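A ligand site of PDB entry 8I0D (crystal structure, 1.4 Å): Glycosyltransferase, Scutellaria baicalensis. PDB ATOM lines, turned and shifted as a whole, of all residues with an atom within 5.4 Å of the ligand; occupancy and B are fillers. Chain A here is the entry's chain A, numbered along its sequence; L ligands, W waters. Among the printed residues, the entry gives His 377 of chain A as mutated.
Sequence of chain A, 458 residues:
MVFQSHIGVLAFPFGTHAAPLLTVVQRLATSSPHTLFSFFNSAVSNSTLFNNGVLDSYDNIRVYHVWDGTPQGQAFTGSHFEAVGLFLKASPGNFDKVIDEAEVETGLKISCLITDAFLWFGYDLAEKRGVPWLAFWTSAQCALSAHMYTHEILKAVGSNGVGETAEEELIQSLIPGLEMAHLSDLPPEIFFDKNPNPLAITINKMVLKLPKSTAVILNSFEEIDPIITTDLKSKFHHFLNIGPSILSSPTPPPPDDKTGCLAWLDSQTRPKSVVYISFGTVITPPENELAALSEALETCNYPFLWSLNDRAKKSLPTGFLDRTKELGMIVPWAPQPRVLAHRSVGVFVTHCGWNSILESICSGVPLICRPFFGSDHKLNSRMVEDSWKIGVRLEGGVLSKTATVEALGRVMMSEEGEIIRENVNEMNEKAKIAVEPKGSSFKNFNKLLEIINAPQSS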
ATOM      1  N   PHE A  14     -13.842 -18.485 -19.898  1.00  0.00           N
ATOM      2  CA  PHE A  14     -14.903 -19.444 -19.510  1.00  0.00           C
ATOM      3  C   PHE A  14     -15.642 -18.934 -18.286  1.00  0.00           C
ATOM      4  O   PHE A  14     -15.121 -18.224 -17.527  1.00  0.00           O
ATOM      5  CB  PHE A  14     -14.234 -20.771 -19.222  1.00  0.00           C
ATOM      6  CG  PHE A  14     -13.459 -21.320 -20.383  1.00  0.00           C
ATOM      7  CD1 PHE A  14     -14.138 -21.882 -21.479  1.00  0.00           C
ATOM      8  CD2 PHE A  14     -12.090 -21.222 -20.438  1.00  0.00           C
ATOM      9  CE1 PHE A  14     -13.432 -22.377 -22.559  1.00  0.00           C
ATOM     10  CE2 PHE A  14     -11.390 -21.750 -21.529  1.00  0.00           C
ATOM     11  CZ  PHE A  14     -12.062 -22.301 -22.584  1.00  0.00           C
ATOM     12  N   GLY A  15     -16.868 -19.451 -18.038  1.00  0.00           N
ATOM     13  CA  GLY A  15     -17.651 -19.025 -16.895  1.00  0.00           C
ATOM     14  C   GLY A  15     -17.933 -17.536 -16.938  1.00  0.00           C
ATOM     15  O   GLY A  15     -17.879 -16.973 -18.019  1.00  0.00           O
ATOM     16  N   THR A  16     -18.065 -16.898 -15.783  1.00  0.00           N
ATOM     17  CA  THR A  16     -18.377 -15.452 -15.677  1.00  0.00           C
ATOM     18  C   THR A  16     -17.073 -14.731 -15.344  1.00  0.00           C
ATOM     19  O   THR A  16     -17.031 -14.083 -14.313  1.00  0.00           O
ATOM     20  CB  THR A  16     -19.455 -15.221 -14.629  1.00  0.00           C
ATOM     21  OG1 THR A  16     -19.072 -15.923 -13.464  1.00  0.00           O
ATOM     22  CG2 THR A  16     -20.738 -15.836 -15.054  1.00  0.00           C
ATOM     23  N   HIS A  17     -16.001 -15.099 -16.027  1.00  0.00           N
ATOM     24  CA  HIS A  17     -14.688 -14.497 -15.710  1.00  0.00           C
ATOM     25  C   HIS A  17     -14.398 -13.232 -16.559  1.00  0.00           C
ATOM     26  O   HIS A  17     -13.811 -12.278 -16.054  1.00  0.00           O
ATOM     27  CB  HIS A  17     -13.567 -15.500 -15.939  1.00  0.00           C
ATOM     28  CG  HIS A  17     -13.365 -16.488 -14.857  1.00  0.00           C
ATOM     29  ND1 HIS A  17     -12.305 -16.474 -14.016  1.00  0.00           N
ATOM     30  CD2 HIS A  17     -14.048 -17.607 -14.534  1.00  0.00           C
ATOM     31  CE1 HIS A  17     -12.354 -17.511 -13.182  1.00  0.00           C
ATOM     32  NE2 HIS A  17     -13.439 -18.235 -13.470  1.00  0.00           N
ATOM     33  N   THR A 138     -11.865 -13.251  -9.381  1.00  0.00           N
ATOM     34  CA  THR A 138     -13.246 -13.033  -9.819  1.00  0.00           C
ATOM     35  C   THR A 138     -14.296 -13.411  -8.764  1.00  0.00           C
ATOM     36  O   THR A 138     -15.477 -13.272  -9.063  1.00  0.00           O
ATOM     37  CB  THR A 138     -13.519 -13.780 -11.107  1.00  0.00           C
ATOM     38  OG1 THR A 138     -13.375 -15.166 -10.888  1.00  0.00           O
ATOM     39  CG2 THR A 138     -12.662 -13.337 -12.276  1.00  0.00           C
ATOM     40  N   SER A 139     -13.899 -13.781  -7.566  1.00  0.00           N
ATOM     41  CA  SER A 139     -14.782 -14.149  -6.441  1.00  0.00           C
ATOM     42  C   SER A 139     -14.562 -13.249  -5.218  1.00  0.00           C
ATOM     43  O   SER A 139     -13.974 -12.168  -5.334  1.00  0.00           O
ATOM     44  CB  SER A 139     -14.574 -15.689  -6.068  1.00  0.00           C
ATOM     45  OG  SER A 139     -14.923 -16.482  -7.158  1.00  0.00           O
ATOM     46  N   ALA A 140     -15.033 -13.657  -4.038  1.00  0.00           N
ATOM     47  CA  ALA A 140     -14.892 -12.832  -2.842  1.00  0.00           C
ATOM     48  C   ALA A 140     -13.597 -13.188  -2.124  1.00  0.00           C
ATOM     49  O   ALA A 140     -12.924 -14.216  -2.476  1.00  0.00           O
ATOM     50  CB  ALA A 140     -16.071 -13.074  -1.971  1.00  0.00           C
ATOM     51  N   TYR A 276     -37.590 -14.145  -6.343  1.00  0.00           N
ATOM     52  CA  TYR A 276     -36.829 -14.252  -7.609  1.00  0.00           C
ATOM     53  C   TYR A 276     -35.916 -15.484  -7.533  1.00  0.00           C
ATOM     54  O   TYR A 276     -35.329 -15.749  -6.473  1.00  0.00           O
ATOM     55  CB  TYR A 276     -35.985 -12.995  -7.815  1.00  0.00           C
ATOM     56  CG  TYR A 276     -35.047 -13.133  -8.980  1.00  0.00           C
ATOM     57  CD1 TYR A 276     -35.525 -13.266 -10.273  1.00  0.00           C
ATOM     58  CD2 TYR A 276     -33.673 -13.178  -8.769  1.00  0.00           C
ATOM     59  CE1 TYR A 276     -34.649 -13.440 -11.333  1.00  0.00           C
ATOM     60  CE2 TYR A 276     -32.798 -13.305  -9.843  1.00  0.00           C
ATOM     61  CZ  TYR A 276     -33.281 -13.448 -11.118  1.00  0.00           C
ATOM     62  OH  TYR A 276     -32.443 -13.601 -12.188  1.00  0.00           O
ATOM     63  N   SER A 278     -33.091 -17.823  -9.597  1.00  0.00           N
ATOM     64  CA  SER A 278     -32.150 -18.098 -10.687  1.00  0.00           C
ATOM     65  C   SER A 278     -31.005 -18.974 -10.162  1.00  0.00           C
ATOM     66  O   SER A 278     -30.459 -18.685  -9.121  1.00  0.00           O
ATOM     67  CB  SER A 278     -31.642 -16.820 -11.233  1.00  0.00           C
ATOM     68  OG  SER A 278     -30.680 -17.077 -12.257  1.00  0.00           O
ATOM     69  N   GLY A 280     -28.220 -19.292 -12.143  1.00  0.00           N
ATOM     70  CA  GLY A 280     -27.059 -18.915 -12.986  1.00  0.00           C
ATOM     71  C   GLY A 280     -27.310 -19.240 -14.429  1.00  0.00           C
ATOM     72  O   GLY A 280     -28.445 -19.515 -14.769  1.00  0.00           O
ATOM     73  N   THR A 281     -26.261 -19.214 -15.233  1.00  0.00           N
ATOM     74  CA  THR A 281     -26.341 -19.304 -16.712  1.00  0.00           C
ATOM     75  C   THR A 281     -26.252 -20.777 -17.147  1.00  0.00           C
ATOM     76  O   THR A 281     -26.596 -21.057 -18.304  1.00  0.00           O
ATOM     77  CB  THR A 281     -25.253 -18.434 -17.372  1.00  0.00           C
ATOM     78  OG1 THR A 281     -23.905 -18.868 -17.026  1.00  0.00           O
ATOM     79  CG2 THR A 281     -25.338 -17.009 -16.960  1.00  0.00           C
ATOM     80  N   SER A 307     -36.068 -17.414 -13.558  1.00  0.00           N
ATOM     81  CA  SER A 307     -35.180 -17.561 -14.727  1.00  0.00           C
ATOM     82  C   SER A 307     -34.901 -19.055 -14.894  1.00  0.00           C
ATOM     83  O   SER A 307     -34.219 -19.675 -14.062  1.00  0.00           O
ATOM     84  CB  SER A 307     -33.950 -16.743 -14.597  1.00  0.00           C
ATOM     85  OG  SER A 307     -33.159 -16.849 -15.750  1.00  0.00           O
ATOM     86  N   PRO A 332     -36.690 -17.421 -19.881  1.00  0.00           N
ATOM     87  CA  PRO A 332     -35.422 -18.120 -20.060  1.00  0.00           C
ATOM     88  C   PRO A 332     -34.208 -17.274 -19.609  1.00  0.00           C
ATOM     89  O   PRO A 332     -33.119 -17.787 -19.380  1.00  0.00           O
ATOM     90  CB  PRO A 332     -35.435 -18.428 -21.569  1.00  0.00           C
ATOM     91  CG  PRO A 332     -36.239 -17.289 -22.174  1.00  0.00           C
ATOM     92  CD  PRO A 332     -37.304 -16.979 -21.146  1.00  0.00           C
ATOM     93  N   TRP A 333     -34.419 -15.972 -19.457  1.00  0.00           N
ATOM     94  CA  TRP A 333     -33.365 -15.014 -19.058  1.00  0.00           C
ATOM     95  C   TRP A 333     -34.008 -13.753 -18.475  1.00  0.00           C
ATOM     96  O   TRP A 333     -34.948 -13.237 -19.061  1.00  0.00           O
ATOM     97  CB  TRP A 333     -32.436 -14.662 -20.216  1.00  0.00           C
ATOM     98  CG  TRP A 333     -31.273 -13.771 -19.858  1.00  0.00           C
ATOM     99  CD1 TRP A 333     -30.049 -14.160 -19.398  1.00  0.00           C
ATOM    100  CD2 TRP A 333     -31.233 -12.334 -19.875  1.00  0.00           C
ATOM    101  NE1 TRP A 333     -29.234 -13.087 -19.210  1.00  0.00           N
ATOM    102  CE2 TRP A 333     -29.936 -11.935 -19.474  1.00  0.00           C
ATOM    103  CE3 TRP A 333     -32.183 -11.350 -20.209  1.00  0.00           C
ATOM    104  CZ2 TRP A 333     -29.567 -10.595 -19.382  1.00  0.00           C
ATOM    105  CZ3 TRP A 333     -31.817 -10.005 -20.093  1.00  0.00           C
ATOM    106  CH2 TRP A 333     -30.514  -9.643 -19.696  1.00  0.00           C
ATOM    107  N   ALA A 334     -33.490 -13.314 -17.335  1.00  0.00           N
ATOM    108  CA  ALA A 334     -33.943 -12.085 -16.658  1.00  0.00           C
ATOM    109  C   ALA A 334     -32.823 -11.077 -16.620  1.00  0.00           C
ATOM    110  O   ALA A 334     -31.664 -11.430 -16.538  1.00  0.00           O
ATOM    111  CB  ALA A 334     -34.465 -12.399 -15.264  1.00  0.00           C
ATOM    112  N   PRO A 335     -33.157  -9.773 -16.672  1.00  0.00           N
ATOM    113  CA  PRO A 335     -32.179  -8.709 -16.466  1.00  0.00           C
ATOM    114  C   PRO A 335     -31.917  -8.626 -14.967  1.00  0.00           C
ATOM    115  O   PRO A 335     -32.449  -7.772 -14.249  1.00  0.00           O
ATOM    116  CB  PRO A 335     -32.863  -7.473 -17.074  1.00  0.00           C
ATOM    117  CG  PRO A 335     -34.337  -7.749 -16.833  1.00  0.00           C
ATOM    118  CD  PRO A 335     -34.519  -9.252 -16.955  1.00  0.00           C
ATOM    119  N   GLN A 336     -31.092  -9.551 -14.463  1.00  0.00           N
ATOM    120  CA  GLN A 336     -31.087  -9.888 -13.011  1.00  0.00           C
ATOM    121  C   GLN A 336     -30.793  -8.655 -12.170  1.00  0.00           C
ATOM    122  O   GLN A 336     -31.444  -8.471 -11.142  1.00  0.00           O
ATOM    123  CB  GLN A 336     -30.164 -11.073 -12.742  1.00  0.00           C
ATOM    124  CG  GLN A 336     -29.899 -11.288 -11.270  1.00  0.00           C
ATOM    125  CD  GLN A 336     -29.282 -12.628 -10.973  1.00  0.00           C
ATOM    126  OE1 GLN A 336     -29.806 -13.656 -11.395  1.00  0.00           O
ATOM    127  NE2 GLN A 336     -28.118 -12.605 -10.311  1.00  0.00           N
ATOM    128  N   PRO A 337     -29.735  -7.851 -12.436  1.00  0.00           N
ATOM    129  CA  PRO A 337     -29.514  -6.689 -11.568  1.00  0.00           C
ATOM    130  C   PRO A 337     -30.736  -5.754 -11.476  1.00  0.00           C
ATOM    131  O   PRO A 337     -30.967  -5.215 -10.401  1.00  0.00           O
ATOM    132  CB  PRO A 337     -28.310  -5.966 -12.212  1.00  0.00           C
ATOM    133  CG  PRO A 337     -27.602  -7.074 -12.996  1.00  0.00           C
ATOM    134  CD  PRO A 337     -28.688  -8.020 -13.451  1.00  0.00           C
ATOM    135  N   HIS A 351     -28.071 -20.020  -6.681  1.00  0.00           N
ATOM    136  CA  HIS A 351     -26.996 -21.052  -6.661  1.00  0.00           C
ATOM    137  C   HIS A 351     -25.715 -20.543  -5.966  1.00  0.00           C
ATOM    138  O   HIS A 351     -24.772 -21.310  -5.801  1.00  0.00           O
ATOM    139  CB  HIS A 351     -26.676 -21.528  -8.055  1.00  0.00           C
ATOM    140  CG  HIS A 351     -25.816 -20.607  -8.804  1.00  0.00           C
ATOM    141  ND1 HIS A 351     -26.121 -19.264  -8.991  1.00  0.00           N
ATOM    142  CD2 HIS A 351     -24.712 -20.856  -9.471  1.00  0.00           C
ATOM    143  CE1 HIS A 351     -25.166 -18.692  -9.722  1.00  0.00           C
ATOM    144  NE2 HIS A 351     -24.292 -19.707 -10.047  1.00  0.00           N
ATOM    145  N   CYS A 352     -25.676 -19.304  -5.482  1.00  0.00           N
ATOM    146  CA  CYS A 352     -24.609 -18.753  -4.634  1.00  0.00           C
ATOM    147  C   CYS A 352     -23.348 -18.472  -5.444  1.00  0.00           C
ATOM    148  O   CYS A 352     -22.287 -18.361  -4.847  1.00  0.00           O
ATOM    149  CB  CYS A 352     -24.241 -19.644  -3.484  1.00  0.00           C
ATOM    150  SG  CYS A 352     -25.660 -19.995  -2.434  1.00  0.00           S
ATOM    151  N   GLY A 353     -23.497 -18.178  -6.708  1.00  0.00           N
ATOM    152  CA  GLY A 353     -22.426 -17.546  -7.475  1.00  0.00           C
ATOM    153  C   GLY A 353     -22.105 -16.186  -6.889  1.00  0.00           C
ATOM    154  O   GLY A 353     -23.028 -15.479  -6.441  1.00  0.00           O
ATOM    155  N   TRP A 354     -20.845 -15.800  -6.902  1.00  0.00           N
ATOM    156  CA  TRP A 354     -20.449 -14.518  -6.286  1.00  0.00           C
ATOM    157  C   TRP A 354     -21.155 -13.334  -6.948  1.00  0.00           C
ATOM    158  O   TRP A 354     -21.589 -12.445  -6.200  1.00  0.00           O
ATOM    159  CB  TRP A 354     -18.946 -14.332  -6.360  1.00  0.00           C
ATOM    160  CG  TRP A 354     -18.485 -12.994  -5.857  1.00  0.00           C
ATOM    161  CD1 TRP A 354     -17.836 -12.048  -6.593  1.00  0.00           C
ATOM    162  CD2 TRP A 354     -18.755 -12.404  -4.575  1.00  0.00           C
ATOM    163  NE1 TRP A 354     -17.607 -10.956  -5.814  1.00  0.00           N
ATOM    164  CE2 TRP A 354     -18.141 -11.152  -4.568  1.00  0.00           C
ATOM    165  CE3 TRP A 354     -19.412 -12.838  -3.424  1.00  0.00           C
ATOM    166  CZ2 TRP A 354     -18.213 -10.306  -3.463  1.00  0.00           C
ATOM    167  CZ3 TRP A 354     -19.517 -11.984  -2.363  1.00  0.00           C
ATOM    168  CH2 TRP A 354     -18.915 -10.727  -2.363  1.00  0.00           C
ATOM    169  N   ASN A 355     -21.235 -13.262  -8.264  1.00  0.00           N
ATOM    170  CA  ASN A 355     -21.817 -12.061  -8.893  1.00  0.00           C
ATOM    171  C   ASN A 355     -23.284 -11.953  -8.457  1.00  0.00           C
ATOM    172  O   ASN A 355     -23.772 -10.850  -8.207  1.00  0.00           O
ATOM    173  CB  ASN A 355     -21.673 -11.995 -10.404  1.00  0.00           C
ATOM    174  CG  ASN A 355     -20.207 -11.936 -10.750  1.00  0.00           C
ATOM    175  OD1 ASN A 355     -19.574 -10.904 -10.627  1.00  0.00           O
ATOM    176  ND2 ASN A 355     -19.651 -13.070 -11.110  1.00  0.00           N
ATOM    177  N   SER A 356     -23.978 -13.074  -8.388  1.00  0.00           N
ATOM    178  CA  SER A 356     -25.387 -13.063  -7.965  1.00  0.00           C
ATOM    179  C   SER A 356     -25.490 -12.581  -6.517  1.00  0.00           C
ATOM    180  O   SER A 356     -26.399 -11.752  -6.185  1.00  0.00           O
ATOM    181  CB  SER A 356     -26.011 -14.414  -8.137  1.00  0.00           C
ATOM    182  OG  SER A 356     -26.187 -14.744  -9.489  1.00  0.00           O
ATOM    183  N   ILE A 357     -24.681 -13.090  -5.599  1.00  0.00           N
ATOM    184  CA  ILE A 357     -24.685 -12.650  -4.205  1.00  0.00           C
ATOM    185  C   ILE A 357     -24.407 -11.162  -4.144  1.00  0.00           C
ATOM    186  O   ILE A 357     -25.088 -10.434  -3.376  1.00  0.00           O
ATOM    187  CB  ILE A 357     -23.788 -13.496  -3.339  1.00  0.00           C
ATOM    188  CG1 ILE A 357     -24.414 -14.906  -3.196  1.00  0.00           C
ATOM    189  CG2 ILE A 357     -23.519 -12.830  -1.989  1.00  0.00           C
ATOM    190  CD1 ILE A 357     -23.421 -15.903  -2.597  1.00  0.00           C
ATOM    191  N   GLU A 359     -24.776  -8.842  -6.399  1.00  0.00           N
ATOM    192  CA  GLU A 359     -25.935  -8.082  -6.939  1.00  0.00           C
ATOM    193  C   GLU A 359     -27.023  -7.986  -5.868  1.00  0.00           C
ATOM    194  O   GLU A 359     -27.732  -6.960  -5.756  1.00  0.00           O
ATOM    195  CB  GLU A 359     -26.426  -8.715  -8.236  1.00  0.00           C
ATOM    196  CG  GLU A 359     -25.433  -8.527  -9.355  1.00  0.00           C
ATOM    197  CD  GLU A 359     -25.599  -9.512 -10.498  1.00  0.00           C
ATOM    198  OE1 GLU A 359     -26.620 -10.247 -10.557  1.00  0.00           O
ATOM    199  OE2 GLU A 359     -24.629  -9.613 -11.301  1.00  0.00           O
ATOM    200  N   SER A 375     -16.296 -24.967  -7.384  1.00  0.00           N
ATOM    201  CA  SER A 375     -15.989 -23.533  -7.228  1.00  0.00           C
ATOM    202  C   SER A 375     -16.271 -23.153  -5.767  1.00  0.00           C
ATOM    203  O   SER A 375     -16.108 -23.962  -4.837  1.00  0.00           O
ATOM    204  CB  SER A 375     -16.854 -22.757  -8.256  1.00  0.00           C
ATOM    205  OG  SER A 375     -16.451 -21.422  -8.335  1.00  0.00           O
ATOM    206  N   ASP A 376     -16.735 -21.950  -5.574  1.00  0.00           N
ATOM    207  CA  ASP A 376     -16.860 -21.342  -4.235  1.00  0.00           C
ATOM    208  C   ASP A 376     -18.352 -21.315  -3.818  1.00  0.00           C
ATOM    209  O   ASP A 376     -18.655 -20.651  -2.825  1.00  0.00           O
ATOM    210  CB  ASP A 376     -16.314 -19.923  -4.290  1.00  0.00           C
ATOM    211  CG  ASP A 376     -17.090 -19.036  -5.271  1.00  0.00           C
ATOM    212  OD1 ASP A 376     -17.858 -19.540  -6.004  1.00  0.00           O
ATOM    213  OD2 ASP A 376     -16.895 -17.786  -5.304  1.00  0.00           O
ATOM    214  N   HIS A 377     -19.244 -22.041  -4.485  1.00  0.00           N
ATOM    215  CA  HIS A 377     -20.694 -21.850  -4.237  1.00  0.00           C
ATOM    216  C   HIS A 377     -21.027 -22.320  -2.840  1.00  0.00           C
ATOM    217  O   HIS A 377     -21.751 -21.624  -2.121  1.00  0.00           O
ATOM    218  CB  HIS A 377     -21.500 -22.549  -5.315  1.00  0.00           C
ATOM    219  CG  HIS A 377     -21.209 -21.987  -6.669  1.00  0.00           C
ATOM    220  ND1 HIS A 377     -20.910 -22.749  -7.701  1.00  0.00           N
ATOM    221  CD2 HIS A 377     -21.138 -20.755  -7.114  1.00  0.00           C
ATOM    222  CE1 HIS A 377     -20.695 -22.017  -8.782  1.00  0.00           C
ATOM    223  NE2 HIS A 377     -20.813 -20.788  -8.433  1.00  0.00           N
ATOM    224  N   ASN A 380     -19.658 -19.866  -0.284  1.00  0.00           N
ATOM    225  CA  ASN A 380     -20.475 -18.628  -0.331  1.00  0.00           C
ATOM    226  C   ASN A 380     -21.769 -18.881   0.465  1.00  0.00           C
ATOM    227  O   ASN A 380     -22.192 -18.000   1.233  1.00  0.00           O
ATOM    228  CB  ASN A 380     -20.797 -18.187  -1.711  1.00  0.00           C
ATOM    229  CG  ASN A 380     -19.611 -17.574  -2.405  1.00  0.00           C
ATOM    230  OD1 ASN A 380     -18.622 -17.249  -1.787  1.00  0.00           O
ATOM    231  ND2 ASN A 380     -19.757 -17.428  -3.708  1.00  0.00           N
HETATM  232  N1  LIG L   1     -27.732 -13.609 -14.847  1.00  0.00           N
HETATM  233  C1  LIG L   1     -28.562 -12.788 -15.577  1.00  0.00           C
HETATM  234  N2  LIG L   1     -29.772 -13.321 -15.913  1.00  0.00           N
HETATM  235  C2  LIG L   1     -30.277 -14.567 -15.579  1.00  0.00           C
HETATM  236  C3  LIG L   1     -29.356 -15.385 -14.830  1.00  0.00           C
HETATM  237  C4  LIG L   1     -28.154 -14.876 -14.494  1.00  0.00           C
HETATM  238  O1  LIG L   1     -28.288 -11.644 -15.893  1.00  0.00           O
HETATM  239  O2  LIG L   1     -31.378 -14.882 -16.020  1.00  0.00           O
HETATM  240  C5  LIG L   1     -26.386 -13.106 -14.470  1.00  0.00           C
HETATM  241  C6  LIG L   1     -26.260 -12.616 -13.033  1.00  0.00           C
HETATM  242  O3  LIG L   1     -26.777 -11.294 -12.990  1.00  0.00           O
HETATM  243  C7  LIG L   1     -24.759 -12.744 -12.784  1.00  0.00           C
HETATM  244  C8  LIG L   1     -24.370 -13.941 -13.660  1.00  0.00           C
HETATM  245  O4  LIG L   1     -25.446 -14.168 -14.592  1.00  0.00           O
HETATM  246  O5  LIG L   1     -24.109 -11.523 -13.120  1.00  0.00           O
HETATM  247  C9  LIG L   1     -24.099 -15.234 -12.925  1.00  0.00           C
HETATM  248  O6  LIG L   1     -22.840 -15.059 -12.232  1.00  0.00           O
HETATM  249  P1  LIG L   1     -22.572 -15.723 -10.837  1.00  0.00           P
HETATM  250  O7  LIG L   1     -23.668 -15.493  -9.909  1.00  0.00           O
HETATM  251  O8  LIG L   1     -21.201 -15.260 -10.331  1.00  0.00           O
HETATM  252  O9  LIG L   1     -22.578 -17.282 -11.109  1.00  0.00           O
HETATM  253  P2  LIG L   1     -21.418 -18.303 -11.603  1.00  0.00           P
HETATM  254  O10 LIG L   1     -20.948 -17.812 -12.928  1.00  0.00           O
HETATM  255  O11 LIG L   1     -21.957 -19.661 -11.476  1.00  0.00           O
HETATM  256  O12 LIG L   1     -20.194 -17.968 -10.550  1.00  0.00           O
HETATM  257  C10 LIG L   1     -19.054 -18.737 -10.162  1.00  0.00           C
HETATM  258  C11 LIG L   1     -18.310 -18.087  -8.976  1.00  0.00           C
HETATM  259  C12 LIG L   1     -17.844 -16.728  -9.335  1.00  0.00           C
HETATM  260  C13 LIG L   1     -16.866 -16.829 -10.486  1.00  0.00           C
HETATM  261  C14 LIG L   1     -17.581 -17.524 -11.663  1.00  0.00           C
HETATM  262  C15 LIG L   1     -16.667 -17.810 -12.817  1.00  0.00           C
HETATM  263  O13 LIG L   1     -19.034 -17.885  -7.760  1.00  0.00           O
HETATM  264  O14 LIG L   1     -17.245 -16.183  -8.165  1.00  0.00           O
HETATM  265  O15 LIG L   1     -16.387 -15.539 -10.867  1.00  0.00           O
HETATM  266  O16 LIG L   1     -18.098 -18.827 -11.222  1.00  0.00           O
HETATM  267  O17 LIG L   1     -17.375 -18.531 -13.824  1.00  0.00           O
HETATM  268  O   HOH W   1     -22.657 -21.916 -12.250  1.00  0.00           O
HETATM  269  O   HOH W   2     -25.883  -9.302 -14.920  1.00  0.00           O
HETATM  270  O   HOH W   3     -28.172 -16.052 -11.371  1.00  0.00           O
HETATM  271  O   HOH W   4     -26.802 -13.539 -18.300  1.00  0.00           O
HETATM  272  O   HOH W   5     -21.621 -10.985 -14.454  1.00  0.00           O
HETATM  273  O   HOH W   6     -23.668 -18.302 -13.399  1.00  0.00           O
HETATM  274  O   HOH W   7     -28.097  -8.958 -16.747  1.00  0.00           O
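The side-chain hydroxyl (OG) of Ser 139 sits at hydrogen-bond distance from an oxygen (O14) of the ligand (2.5 Å).
The backbone NH (N) of Thr 16 sits at hydrogen-bond distance from an oxygen (O17) of the ligand, at 2.6 Å.
O10 of the ligand lies within hydrogen-bond range of OG1 of Thr 16, at 2.7 Å.
An oxygen (O3) of the ligand lies within hydrogen-bond range of the side-chain carboxylate (OE1) of Glu 359 (2.7 Å).
An oxygen (O7) of the ligand lies within hydrogen-bond range of the backbone NH (N) of Ser 356 (2.9 Å).
OG of Ser 356 lies within hydrogen-bond range of O7 of the ligand (2.7 Å).
The side-chain hydroxyl (OG) of Ser 307 lies within hydrogen-bond range of an oxygen (O2) of the ligand (2.7 Å).
An oxygen (O13) of the ligand lies within hydrogen-bond range of the side-chain carboxylate (OD1) of Asp 376, at 2.7 Å.
An oxygen (O11) of the ligand sits at hydrogen-bond distance from a ring nitrogen (NE2) of His 351.
N of Ala 334 is in hydrogen-bond range of O2 of the ligand (2.9 Å).
A nitrogen (N2) of the ligand lies within hydrogen-bond range of the backbone carbonyl oxygen (O) of Ala 334.
O8 of the ligand lies within hydrogen-bond range of N of Asn 355 (2.9 Å).
ND2 of Asn 355 sits at hydrogen-bond distance from O8 of the ligand, 2.8 Å away.
N of Trp 354 lies within hydrogen-bond range of O13 of the ligand (2.9 Å).
O15 of the ligand is in hydrogen-bond range of O of Thr 138 (3.0 Å).
OG1 of Thr 138 is in hydrogen-bond range of O15 of the ligand, 3.0 Å away.
A ring nitrogen (NE2) of His 377 lies close to an oxygen (O11) of the ligand, at 3.4 Å.
An oxygen (O3) of the ligand sits at hydrogen-bond distance from the side-chain amide nitrogen (NE2) of Gln 336 (3.3 Å).
Water W6 bridges O9 of the ligand (2.7 Å) and N of Thr 281 (3.3 Å).
Water W4 bridges the indole nitrogen of Trp 333 (2.6 Å) and an oxygen (O1) of the ligand (3.4 Å).
Water W3 lies within hydrogen-bond range of OG of Ser 278 (2.9 Å), OE1 of Gln 336 (2.9 Å), OG of Ser 356 (3.0 Å) and N of Gly 280 (3.3 Å).
The side-chain hydroxyl (OG) of Ser 139 is in hydrogen-bond range of the side-chain carboxylate (OD2) of Asp 376.
The side-chain carboxylate (OE1) of Glu 359 is in hydrogen-bond range of the side-chain amide nitrogen (NE2) of Gln 336 (2.8 Å).
NE2 of Gln 336 lies within hydrogen-bond range of OG of Ser 356 (3.0 Å).
OG of Ser 375 sits at hydrogen-bond distance from OD1 of Asp 376 (3.3 Å).
OD2 of Asp 376 lies within hydrogen-bond range of ND2 of Asn 380.
The side-chain amide oxygen of Gln 336 sits at hydrogen-bond distance from the side-chain hydroxyl of Tyr 276.
N of Gly 280 sits at hydrogen-bond distance from OG of Ser 278 (3.3 Å).
NE1 of Trp 333 sits close to N2 of the ligand (3.3 Å).
Residues that only touch the ligand: Gly 15, His 17, Ser 278, Gly 353, Thr 281, Pro 337 and Ser 375.
Hydrophobic or aromatic side chains within 4 Å of the ligand: His 17, Trp 333, Pro 337, His 351, Trp 354 and His 377.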
